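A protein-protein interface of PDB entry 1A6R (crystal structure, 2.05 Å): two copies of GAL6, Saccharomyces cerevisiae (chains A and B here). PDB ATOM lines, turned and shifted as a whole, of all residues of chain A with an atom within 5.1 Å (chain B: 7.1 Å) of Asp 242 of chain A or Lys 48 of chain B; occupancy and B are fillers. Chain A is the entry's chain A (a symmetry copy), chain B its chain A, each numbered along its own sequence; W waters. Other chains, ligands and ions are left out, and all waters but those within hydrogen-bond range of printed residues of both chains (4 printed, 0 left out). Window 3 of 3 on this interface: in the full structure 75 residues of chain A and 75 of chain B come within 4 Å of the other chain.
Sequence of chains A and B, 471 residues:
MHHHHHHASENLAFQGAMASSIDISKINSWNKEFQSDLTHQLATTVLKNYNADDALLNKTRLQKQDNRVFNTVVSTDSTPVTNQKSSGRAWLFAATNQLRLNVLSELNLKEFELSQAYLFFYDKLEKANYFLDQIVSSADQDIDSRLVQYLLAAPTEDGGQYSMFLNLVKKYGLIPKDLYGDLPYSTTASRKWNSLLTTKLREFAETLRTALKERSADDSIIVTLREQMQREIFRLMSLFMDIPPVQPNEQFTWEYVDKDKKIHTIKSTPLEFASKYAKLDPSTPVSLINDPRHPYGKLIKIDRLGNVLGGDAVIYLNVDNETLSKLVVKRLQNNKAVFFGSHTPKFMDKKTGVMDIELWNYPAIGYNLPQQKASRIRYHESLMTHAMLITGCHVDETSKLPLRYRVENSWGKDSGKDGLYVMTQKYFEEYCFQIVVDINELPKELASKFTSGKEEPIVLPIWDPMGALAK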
ATOM      1  N   PHE A 121      18.929   8.298  17.562  1.00  0.00           N
ATOM      2  CA  PHE A 121      19.463   9.087  18.675  1.00  0.00           C
ATOM      3  C   PHE A 121      20.817   8.542  19.163  1.00  0.00           C
ATOM      4  O   PHE A 121      21.810   9.273  19.255  1.00  0.00           O
ATOM      5  CB  PHE A 121      18.473   9.101  19.849  1.00  0.00           C
ATOM      6  CG  PHE A 121      18.952   9.910  21.032  1.00  0.00           C
ATOM      7  CD1 PHE A 121      18.743  11.277  21.081  1.00  0.00           C
ATOM      8  CD2 PHE A 121      19.660   9.304  22.076  1.00  0.00           C
ATOM      9  CE1 PHE A 121      19.235  12.061  22.150  1.00  0.00           C
ATOM     10  CE2 PHE A 121      20.158  10.075  23.145  1.00  0.00           C
ATOM     11  CZ  PHE A 121      19.948  11.450  23.184  1.00  0.00           C
ATOM     12  N   TYR A 180       8.513   5.669  20.975  1.00  0.00           N
ATOM     13  CA  TYR A 180       9.480   6.721  20.645  1.00  0.00           C
ATOM     14  C   TYR A 180       9.517   6.789  19.120  1.00  0.00           C
ATOM     15  O   TYR A 180      10.040   5.899  18.472  1.00  0.00           O
ATOM     16  CB  TYR A 180      10.838   6.267  21.220  1.00  0.00           C
ATOM     17  CG  TYR A 180      11.953   7.262  21.173  1.00  0.00           C
ATOM     18  CD1 TYR A 180      12.002   8.333  22.060  1.00  0.00           C
ATOM     19  CD2 TYR A 180      12.980   7.123  20.239  1.00  0.00           C
ATOM     20  CE1 TYR A 180      13.052   9.248  22.010  1.00  0.00           C
ATOM     21  CE2 TYR A 180      14.030   8.022  20.182  1.00  0.00           C
ATOM     22  CZ  TYR A 180      14.069   9.072  21.057  1.00  0.00           C
ATOM     23  OH  TYR A 180      15.152   9.910  20.981  1.00  0.00           O
ATOM     24  N   LEU A 183       8.476  12.100  16.130  1.00  0.00           N
ATOM     25  CA  LEU A 183       7.852  13.356  16.494  1.00  0.00           C
ATOM     26  C   LEU A 183       8.802  14.522  16.391  1.00  0.00           C
ATOM     27  O   LEU A 183       8.465  15.528  15.792  1.00  0.00           O
ATOM     28  CB  LEU A 183       7.262  13.304  17.916  1.00  0.00           C
ATOM     29  CG  LEU A 183       5.841  12.771  18.110  1.00  0.00           C
ATOM     30  CD1 LEU A 183       5.487  12.736  19.622  1.00  0.00           C
ATOM     31  CD2 LEU A 183       4.830  13.661  17.320  1.00  0.00           C
ATOM     32  N   PRO A 184      10.028  14.401  16.925  1.00  0.00           N
ATOM     33  CA  PRO A 184      10.908  15.570  16.814  1.00  0.00           C
ATOM     34  C   PRO A 184      11.217  16.021  15.389  1.00  0.00           C
ATOM     35  O   PRO A 184      11.503  15.195  14.515  1.00  0.00           O
ATOM     36  CB  PRO A 184      12.191  15.110  17.504  1.00  0.00           C
ATOM     37  CG  PRO A 184      11.762  13.993  18.366  1.00  0.00           C
ATOM     38  CD  PRO A 184      10.745  13.272  17.530  1.00  0.00           C
ATOM     39  N   TYR A 185      11.256  17.341  15.219  1.00  0.00           N
ATOM     40  CA  TYR A 185      11.567  18.007  13.972  1.00  0.00           C
ATOM     41  C   TYR A 185      12.850  17.445  13.332  1.00  0.00           C
ATOM     42  O   TYR A 185      12.892  17.222  12.125  1.00  0.00           O
ATOM     43  CB  TYR A 185      11.776  19.503  14.246  1.00  0.00           C
ATOM     44  CG  TYR A 185      12.301  20.277  13.054  1.00  0.00           C
ATOM     45  CD1 TYR A 185      11.421  20.796  12.098  1.00  0.00           C
ATOM     46  CD2 TYR A 185      13.679  20.411  12.823  1.00  0.00           C
ATOM     47  CE1 TYR A 185      11.904  21.417  10.927  1.00  0.00           C
ATOM     48  CE2 TYR A 185      14.164  21.011  11.666  1.00  0.00           C
ATOM     49  CZ  TYR A 185      13.262  21.511  10.723  1.00  0.00           C
ATOM     50  OH  TYR A 185      13.712  22.090   9.578  1.00  0.00           O
ATOM     51  N   SER A 238      20.131  16.380  23.524  1.00  0.00           N
ATOM     52  CA  SER A 238      18.874  16.308  24.286  1.00  0.00           C
ATOM     53  C   SER A 238      17.950  17.500  24.017  1.00  0.00           C
ATOM     54  O   SER A 238      16.800  17.480  24.448  1.00  0.00           O
ATOM     55  CB  SER A 238      19.118  16.148  25.813  1.00  0.00           C
ATOM     56  OG  SER A 238      19.708  17.312  26.365  1.00  0.00           O
ATOM     57  N   LEU A 239      18.476  18.552  23.388  1.00  0.00           N
ATOM     58  CA  LEU A 239      17.680  19.717  23.029  1.00  0.00           C
ATOM     59  C   LEU A 239      16.852  19.414  21.777  1.00  0.00           C
ATOM     60  O   LEU A 239      15.737  19.915  21.629  1.00  0.00           O
ATOM     61  CB  LEU A 239      18.572  20.922  22.732  1.00  0.00           C
ATOM     62  CG  LEU A 239      19.374  21.548  23.870  1.00  0.00           C
ATOM     63  CD1 LEU A 239      20.192  22.717  23.340  1.00  0.00           C
ATOM     64  CD2 LEU A 239      18.411  21.981  24.963  1.00  0.00           C
ATOM     65  N   PHE A 240      17.383  18.569  20.892  1.00  0.00           N
ATOM     66  CA  PHE A 240      16.692  18.274  19.641  1.00  0.00           C
ATOM     67  C   PHE A 240      15.903  16.982  19.612  1.00  0.00           C
ATOM     68  O   PHE A 240      14.985  16.823  18.786  1.00  0.00           O
ATOM     69  CB  PHE A 240      17.665  18.398  18.464  1.00  0.00           C
ATOM     70  CG  PHE A 240      18.330  19.759  18.377  1.00  0.00           C
ATOM     71  CD1 PHE A 240      19.408  20.086  19.206  1.00  0.00           C
ATOM     72  CD2 PHE A 240      17.866  20.712  17.502  1.00  0.00           C
ATOM     73  CE1 PHE A 240      20.011  21.331  19.155  1.00  0.00           C
ATOM     74  CE2 PHE A 240      18.468  21.970  17.444  1.00  0.00           C
ATOM     75  CZ  PHE A 240      19.541  22.280  18.275  1.00  0.00           C
ATOM     76  N   MET A 241      16.263  16.056  20.498  1.00  0.00           N
ATOM     77  CA  MET A 241      15.561  14.792  20.652  1.00  0.00           C
ATOM     78  C   MET A 241      15.666  14.428  22.137  1.00  0.00           C
ATOM     79  O   MET A 241      16.592  14.871  22.809  1.00  0.00           O
ATOM     80  CB  MET A 241      16.217  13.691  19.824  1.00  0.00           C
ATOM     81  CG  MET A 241      15.876  13.708  18.323  1.00  0.00           C
ATOM     82  SD  MET A 241      16.578  12.297  17.411  1.00  0.00           S
ATOM     83  CE  MET A 241      15.479  10.954  17.884  1.00  0.00           C
ATOM     84  N   ASP A 242      14.711  13.668  22.662  1.00  0.00           N
ATOM     85  CA  ASP A 242      14.771  13.229  24.062  1.00  0.00           C
ATOM     86  C   ASP A 242      15.596  11.938  24.129  1.00  0.00           C
ATOM     87  O   ASP A 242      15.646  11.186  23.165  1.00  0.00           O
ATOM     88  CB  ASP A 242      13.372  12.862  24.604  1.00  0.00           C
ATOM     89  CG  ASP A 242      12.412  14.014  24.602  1.00  0.00           C
ATOM     90  OD1 ASP A 242      12.843  15.143  24.903  1.00  0.00           O
ATOM     91  OD2 ASP A 242      11.205  13.769  24.320  1.00  0.00           O
ATOM     92  N   ILE A 243      16.193  11.639  25.277  1.00  0.00           N
ATOM     93  CA  ILE A 243      16.916  10.371  25.410  1.00  0.00           C
ATOM     94  C   ILE A 243      15.727   9.402  25.459  1.00  0.00           C
ATOM     95  O   ILE A 243      14.648   9.797  25.911  1.00  0.00           O
ATOM     96  CB  ILE A 243      17.724  10.305  26.773  1.00  0.00           C
ATOM     97  CG1 ILE A 243      18.634   9.061  26.812  1.00  0.00           C
ATOM     98  CG2 ILE A 243      16.755  10.290  27.956  1.00  0.00           C
ATOM     99  CD1 ILE A 243      19.769   9.136  27.860  1.00  0.00           C
ATOM    100  N   PRO A 244      15.854   8.176  24.898  1.00  0.00           N
ATOM    101  CA  PRO A 244      14.721   7.249  24.957  1.00  0.00           C
ATOM    102  C   PRO A 244      14.213   7.086  26.390  1.00  0.00           C
ATOM    103  O   PRO A 244      14.974   7.253  27.362  1.00  0.00           O
ATOM    104  CB  PRO A 244      15.308   5.981  24.379  1.00  0.00           C
ATOM    105  CG  PRO A 244      16.143   6.527  23.296  1.00  0.00           C
ATOM    106  CD  PRO A 244      16.866   7.682  23.946  1.00  0.00           C
ATOM    107  N   ASN B  31      21.043  13.737  31.942  1.00  0.00           N
ATOM    108  CA  ASN B  31      19.697  14.103  31.510  1.00  0.00           C
ATOM    109  C   ASN B  31      18.870  14.603  32.700  1.00  0.00           C
ATOM    110  O   ASN B  31      18.211  15.649  32.622  1.00  0.00           O
ATOM    111  CB  ASN B  31      18.982  12.919  30.859  1.00  0.00           C
ATOM    112  CG  ASN B  31      17.690  13.330  30.221  1.00  0.00           C
ATOM    113  OD1 ASN B  31      17.670  14.220  29.360  1.00  0.00           O
ATOM    114  ND2 ASN B  31      16.592  12.766  30.692  1.00  0.00           N
ATOM    115  N   GLN B  35      17.332  18.436  32.783  1.00  0.00           N
ATOM    116  CA  GLN B  35      15.892  18.606  32.864  1.00  0.00           C
ATOM    117  C   GLN B  35      15.410  19.406  34.073  1.00  0.00           C
ATOM    118  O   GLN B  35      14.257  19.834  34.102  1.00  0.00           O
ATOM    119  CB  GLN B  35      15.187  17.255  32.818  1.00  0.00           C
ATOM    120  CG  GLN B  35      15.272  16.512  31.471  1.00  0.00           C
ATOM    121  CD  GLN B  35      14.690  17.299  30.278  1.00  0.00           C
ATOM    122  OE1 GLN B  35      13.643  17.950  30.393  1.00  0.00           O
ATOM    123  NE2 GLN B  35      15.362  17.218  29.125  1.00  0.00           N
ATOM    124  N   GLN B  41      14.480  22.850  29.945  1.00  0.00           N
ATOM    125  CA  GLN B  41      13.136  22.320  29.728  1.00  0.00           C
ATOM    126  C   GLN B  41      12.456  23.084  28.599  1.00  0.00           C
ATOM    127  O   GLN B  41      11.824  22.485  27.735  1.00  0.00           O
ATOM    128  CB  GLN B  41      12.303  22.472  30.999  1.00  0.00           C
ATOM    129  CG  GLN B  41      12.837  21.701  32.187  1.00  0.00           C
ATOM    130  CD  GLN B  41      12.080  22.024  33.467  1.00  0.00           C
ATOM    131  OE1 GLN B  41      12.624  22.607  34.410  1.00  0.00           O
ATOM    132  NE2 GLN B  41      10.812  21.655  33.500  1.00  0.00           N
ATOM    133  N   LEU B  42      12.588  24.403  28.605  1.00  0.00           N
ATOM    134  CA  LEU B  42      11.977  25.234  27.569  1.00  0.00           C
ATOM    135  C   LEU B  42      12.623  25.008  26.189  1.00  0.00           C
ATOM    136  O   LEU B  42      11.920  24.842  25.180  1.00  0.00           O
ATOM    137  CB  LEU B  42      12.059  26.711  27.945  1.00  0.00           C
ATOM    138  CG  LEU B  42      11.537  27.669  26.851  1.00  0.00           C
ATOM    139  CD1 LEU B  42      10.073  27.366  26.515  1.00  0.00           C
ATOM    140  CD2 LEU B  42      11.692  29.138  27.289  1.00  0.00           C
ATOM    141  N   ALA B  43      13.954  24.986  26.160  1.00  0.00           N
ATOM    142  CA  ALA B  43      14.709  24.799  24.921  1.00  0.00           C
ATOM    143  C   ALA B  43      14.411  23.470  24.237  1.00  0.00           C
ATOM    144  O   ALA B  43      14.184  23.422  23.023  1.00  0.00           O
ATOM    145  CB  ALA B  43      16.216  24.936  25.196  1.00  0.00           C
ATOM    146  N   THR B  44      14.390  22.390  25.010  1.00  0.00           N
ATOM    147  CA  THR B  44      14.119  21.092  24.426  1.00  0.00           C
ATOM    148  C   THR B  44      12.669  20.993  23.908  1.00  0.00           C
ATOM    149  O   THR B  44      12.400  20.276  22.951  1.00  0.00           O
ATOM    150  CB  THR B  44      14.498  19.935  25.387  1.00  0.00           C
ATOM    151  OG1 THR B  44      14.318  18.692  24.713  1.00  0.00           O
ATOM    152  CG2 THR B  44      13.647  19.912  26.615  1.00  0.00           C
ATOM    153  N   THR B  45      11.743  21.738  24.519  1.00  0.00           N
ATOM    154  CA  THR B  45      10.345  21.715  24.073  1.00  0.00           C
ATOM    155  C   THR B  45      10.259  22.368  22.694  1.00  0.00           C
ATOM    156  O   THR B  45       9.751  21.775  21.748  1.00  0.00           O
ATOM    157  CB  THR B  45       9.405  22.471  25.063  1.00  0.00           C
ATOM    158  OG1 THR B  45       9.359  21.757  26.300  1.00  0.00           O
ATOM    159  CG2 THR B  45       7.968  22.530  24.515  1.00  0.00           C
ATOM    160  N   VAL B  46      10.837  23.553  22.580  1.00  0.00           N
ATOM    161  CA  VAL B  46      10.808  24.312  21.349  1.00  0.00           C
ATOM    162  C   VAL B  46      11.594  23.675  20.199  1.00  0.00           C
ATOM    163  O   VAL B  46      11.107  23.588  19.060  1.00  0.00           O
ATOM    164  CB  VAL B  46      11.326  25.744  21.626  1.00  0.00           C
ATOM    165  CG1 VAL B  46      11.316  26.578  20.358  1.00  0.00           C
ATOM    166  CG2 VAL B  46      10.462  26.406  22.695  1.00  0.00           C
ATOM    167  N   LEU B  47      12.790  23.187  20.514  1.00  0.00           N
ATOM    168  CA  LEU B  47      13.699  22.614  19.513  1.00  0.00           C
ATOM    169  C   LEU B  47      13.295  21.290  18.927  1.00  0.00           C
ATOM    170  O   LEU B  47      13.878  20.830  17.938  1.00  0.00           O
ATOM    171  CB  LEU B  47      15.146  22.615  20.014  1.00  0.00           C
ATOM    172  CG  LEU B  47      15.631  24.052  20.247  1.00  0.00           C
ATOM    173  CD1 LEU B  47      17.041  24.062  20.828  1.00  0.00           C
ATOM    174  CD2 LEU B  47      15.553  24.853  18.924  1.00  0.00           C
ATOM    175  N   LYS B  48      12.293  20.674  19.538  1.00  0.00           N
ATOM    176  CA  LYS B  48      11.734  19.439  19.007  1.00  0.00           C
ATOM    177  C   LYS B  48      10.603  19.829  18.028  1.00  0.00           C
ATOM    178  O   LYS B  48      10.127  19.002  17.260  1.00  0.00           O
ATOM    179  CB  LYS B  48      11.146  18.567  20.127  1.00  0.00           C
ATOM    180  CG  LYS B  48      12.182  17.758  20.923  1.00  0.00           C
ATOM    181  CD  LYS B  48      11.518  16.620  21.642  1.00  0.00           C
ATOM    182  CE  LYS B  48      10.669  17.103  22.840  1.00  0.00           C
ATOM    183  NZ  LYS B  48      11.508  17.542  24.007  1.00  0.00           N
ATOM    184  N   ASN B  49      10.235  21.107  18.002  1.00  0.00           N
ATOM    185  CA  ASN B  49       9.111  21.566  17.184  1.00  0.00           C
ATOM    186  C   ASN B  49       9.466  22.324  15.929  1.00  0.00           C
ATOM    187  O   ASN B  49       8.737  22.251  14.960  1.00  0.00           O
ATOM    188  CB  ASN B  49       8.166  22.468  18.010  1.00  0.00           C
ATOM    189  CG  ASN B  49       7.506  21.748  19.168  1.00  0.00           C
ATOM    190  OD1 ASN B  49       7.457  20.521  19.231  1.00  0.00           O
ATOM    191  ND2 ASN B  49       6.960  22.525  20.089  1.00  0.00           N
ATOM    192  N   TYR B  50      10.478  23.175  16.001  1.00  0.00           N
ATOM    193  CA  TYR B  50      10.893  23.984  14.854  1.00  0.00           C
ATOM    194  C   TYR B  50      12.376  23.883  14.605  1.00  0.00           C
ATOM    195  O   TYR B  50      13.146  23.542  15.502  1.00  0.00           O
ATOM    196  CB  TYR B  50      10.572  25.470  15.096  1.00  0.00           C
ATOM    197  CG  TYR B  50       9.104  25.681  15.157  1.00  0.00           C
ATOM    198  CD1 TYR B  50       8.370  25.821  13.984  1.00  0.00           C
ATOM    199  CD2 TYR B  50       8.406  25.528  16.365  1.00  0.00           C
ATOM    200  CE1 TYR B  50       6.992  25.776  13.999  1.00  0.00           C
ATOM    201  CE2 TYR B  50       7.023  25.476  16.390  1.00  0.00           C
ATOM    202  CZ  TYR B  50       6.319  25.593  15.199  1.00  0.00           C
ATOM    203  OH  TYR B  50       4.952  25.448  15.181  1.00  0.00           O
ATOM    204  N   ASN B  51      12.765  24.257  13.397  1.00  0.00           N
ATOM    205  CA  ASN B  51      14.158  24.300  12.986  1.00  0.00           C
ATOM    206  C   ASN B  51      14.819  25.321  13.948  1.00  0.00           C
ATOM    207  O   ASN B  51      14.218  26.359  14.253  1.00  0.00           O
ATOM    208  CB  ASN B  51      14.190  24.822  11.549  1.00  0.00           C
ATOM    209  CG  ASN B  51      15.558  24.742  10.931  1.00  0.00           C
ATOM    210  OD1 ASN B  51      16.416  25.581  11.183  1.00  0.00           O
ATOM    211  ND2 ASN B  51      15.780  23.718  10.132  1.00  0.00           N
HETATM  212  O   HOH W   1      14.383  18.377  16.735  1.00  0.00           O
HETATM  213  O   HOH W   2      17.852  16.870  28.681  1.00  0.00           O
HETATM  214  O   HOH W   3      15.878  13.889  27.142  1.00  0.00           O
HETATM  215  O   HOH W   4      15.307  16.236  26.142  1.00  0.00           O
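The side-chain hydroxyl (OG1) of Thr 44 of chain B sits at hydrogen-bond distance from the backbone carbonyl oxygen (O) of Ser 238 of chain A (2.8 Å).
O of Lys 48 of chain B lies within hydrogen-bond range of N of Tyr 185 of chain A (2.9 Å).
NZ of Lys 48 of chain B lies within salt-bridge range of OD1 of Asp 242 of chain A (2.9 Å).
The side-chain hydroxyl of Tyr 185 of chain A lies within hydrogen-bond range of the side-chain amide nitrogen of Asn 51 of chain B, at 2.7 Å.
The backbone carbonyl oxygen (O) of Thr 44 of chain B sits at hydrogen-bond distance from the side-chain amino group (NZ) of Lys 48 of chain B.
The backbone carbonyl oxygen (O) of Asp 242 of chain A lies within hydrogen-bond range of the side-chain hydroxyl (OH) of Tyr 180 of chain A.
Among the printed residues, merely in contact across the chains: Pro 184 of chain A with Lys 48 of chain B (3.5 Å), Tyr 185 of chain A with Tyr 50 of chain B (3.9 Å), Leu 239 of chain A with Ala 43 of chain B (3.7 Å), Leu 239 of chain A with Thr 44 of chain B (3.4 Å), Leu 239 of chain A with Leu 47 of chain B (3.2 Å), Phe 240 of chain A with Leu 47 of chain B (3.99 Å), Phe 240 of chain A with Lys 48 of chain B (3.6 Å), Asp 242 of chain A with Thr 44 of chain B (3.8 Å) and Ile 243 of chain A with Asn 31 of chain B (3.7 Å).
Tyr 180 of chain A touches none of the printed residues of chain B.
Leu 183 of chain A touches none of the printed residues of chain B.
Printed residues of chain B within 4 Å of Ser 238 of chain A: Thr 44.
Of the printed residues of chain B, Leu 239 of chain A touches Ala 43 (3.7 Å), Thr 44 (3.4 Å) and Leu 47 (3.2 Å).
Of chain B, only Thr 44 and Lys 48 come within 4 Å of Asp 242 of chain A.
Printed residues of chain A within 4 Å of Leu 47 of chain B: Leu 239 and Phe 240.
Lys 48 of chain B touches just these residues of chain A: Pro 184, Tyr 185, Phe 240 and Asp 242.
Printed residues of chain A within 4 Å of Tyr 50 of chain B: Tyr 185.
The nearest residue of chain B that does not touch Asp 242 of chain A is Gln 35 of chain B (5.3 Å).
The nearest printed residue of chain A that does not touch Lys 48 of chain B is Leu 239 of chain A (4.1 Å).
Of the 13 printed residues of chain B, 7 touch a printed residue of chain A.
Printed residues of chain B that touch a printed residue of chain A: Asn 31, Ala 43, Thr 44, Leu 47, Lys 48, Tyr 50 and Asn 51.
Along chain B the printed residues that touch a printed residue of chain A span positions 31 to 51.
Among the printed residues, 13 pairs touch across the chains.
Among the printed residues, Asp or Glu carboxylates within 4 Å of a Lys or Arg side-chain nitrogen of the other chain: Asp 242 of chain A with Lys 48 of chain B.
No position is printed for both chains.
Of the 13 pairs that touch across the chains among the printed residues, none has its exchanged pair printed and touching as well.
Water W2 lies within hydrogen-bond range of the side-chain amide nitrogen (NE2) of Gln 35 of chain B, the side-chain amide oxygen (OD1) of Asn 31 of chain B and the side-chain hydroxyl (OG) of Ser 238 of chain A.
Water W4 lies within hydrogen-bond range of the backbone carbonyl oxygen of Ser 238 of chain A (2.6 Å), the side-chain carboxylate of Asp 242 of chain A (3.0 Å), the side-chain hydroxyl of Thr 44 of chain B (3.0 Å) and the side-chain amide nitrogen of Gln 35 of chain B (3.1 Å).
Water W1 bridges the backbone carbonyl oxygen (O) of Phe 240 of chain A and the backbone carbonyl oxygen (O) of Leu 47 of chain B.
Water W3 lies within hydrogen-bond range of OD1 of Asn 31 of chain B and N of Ile 243 of chain A.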
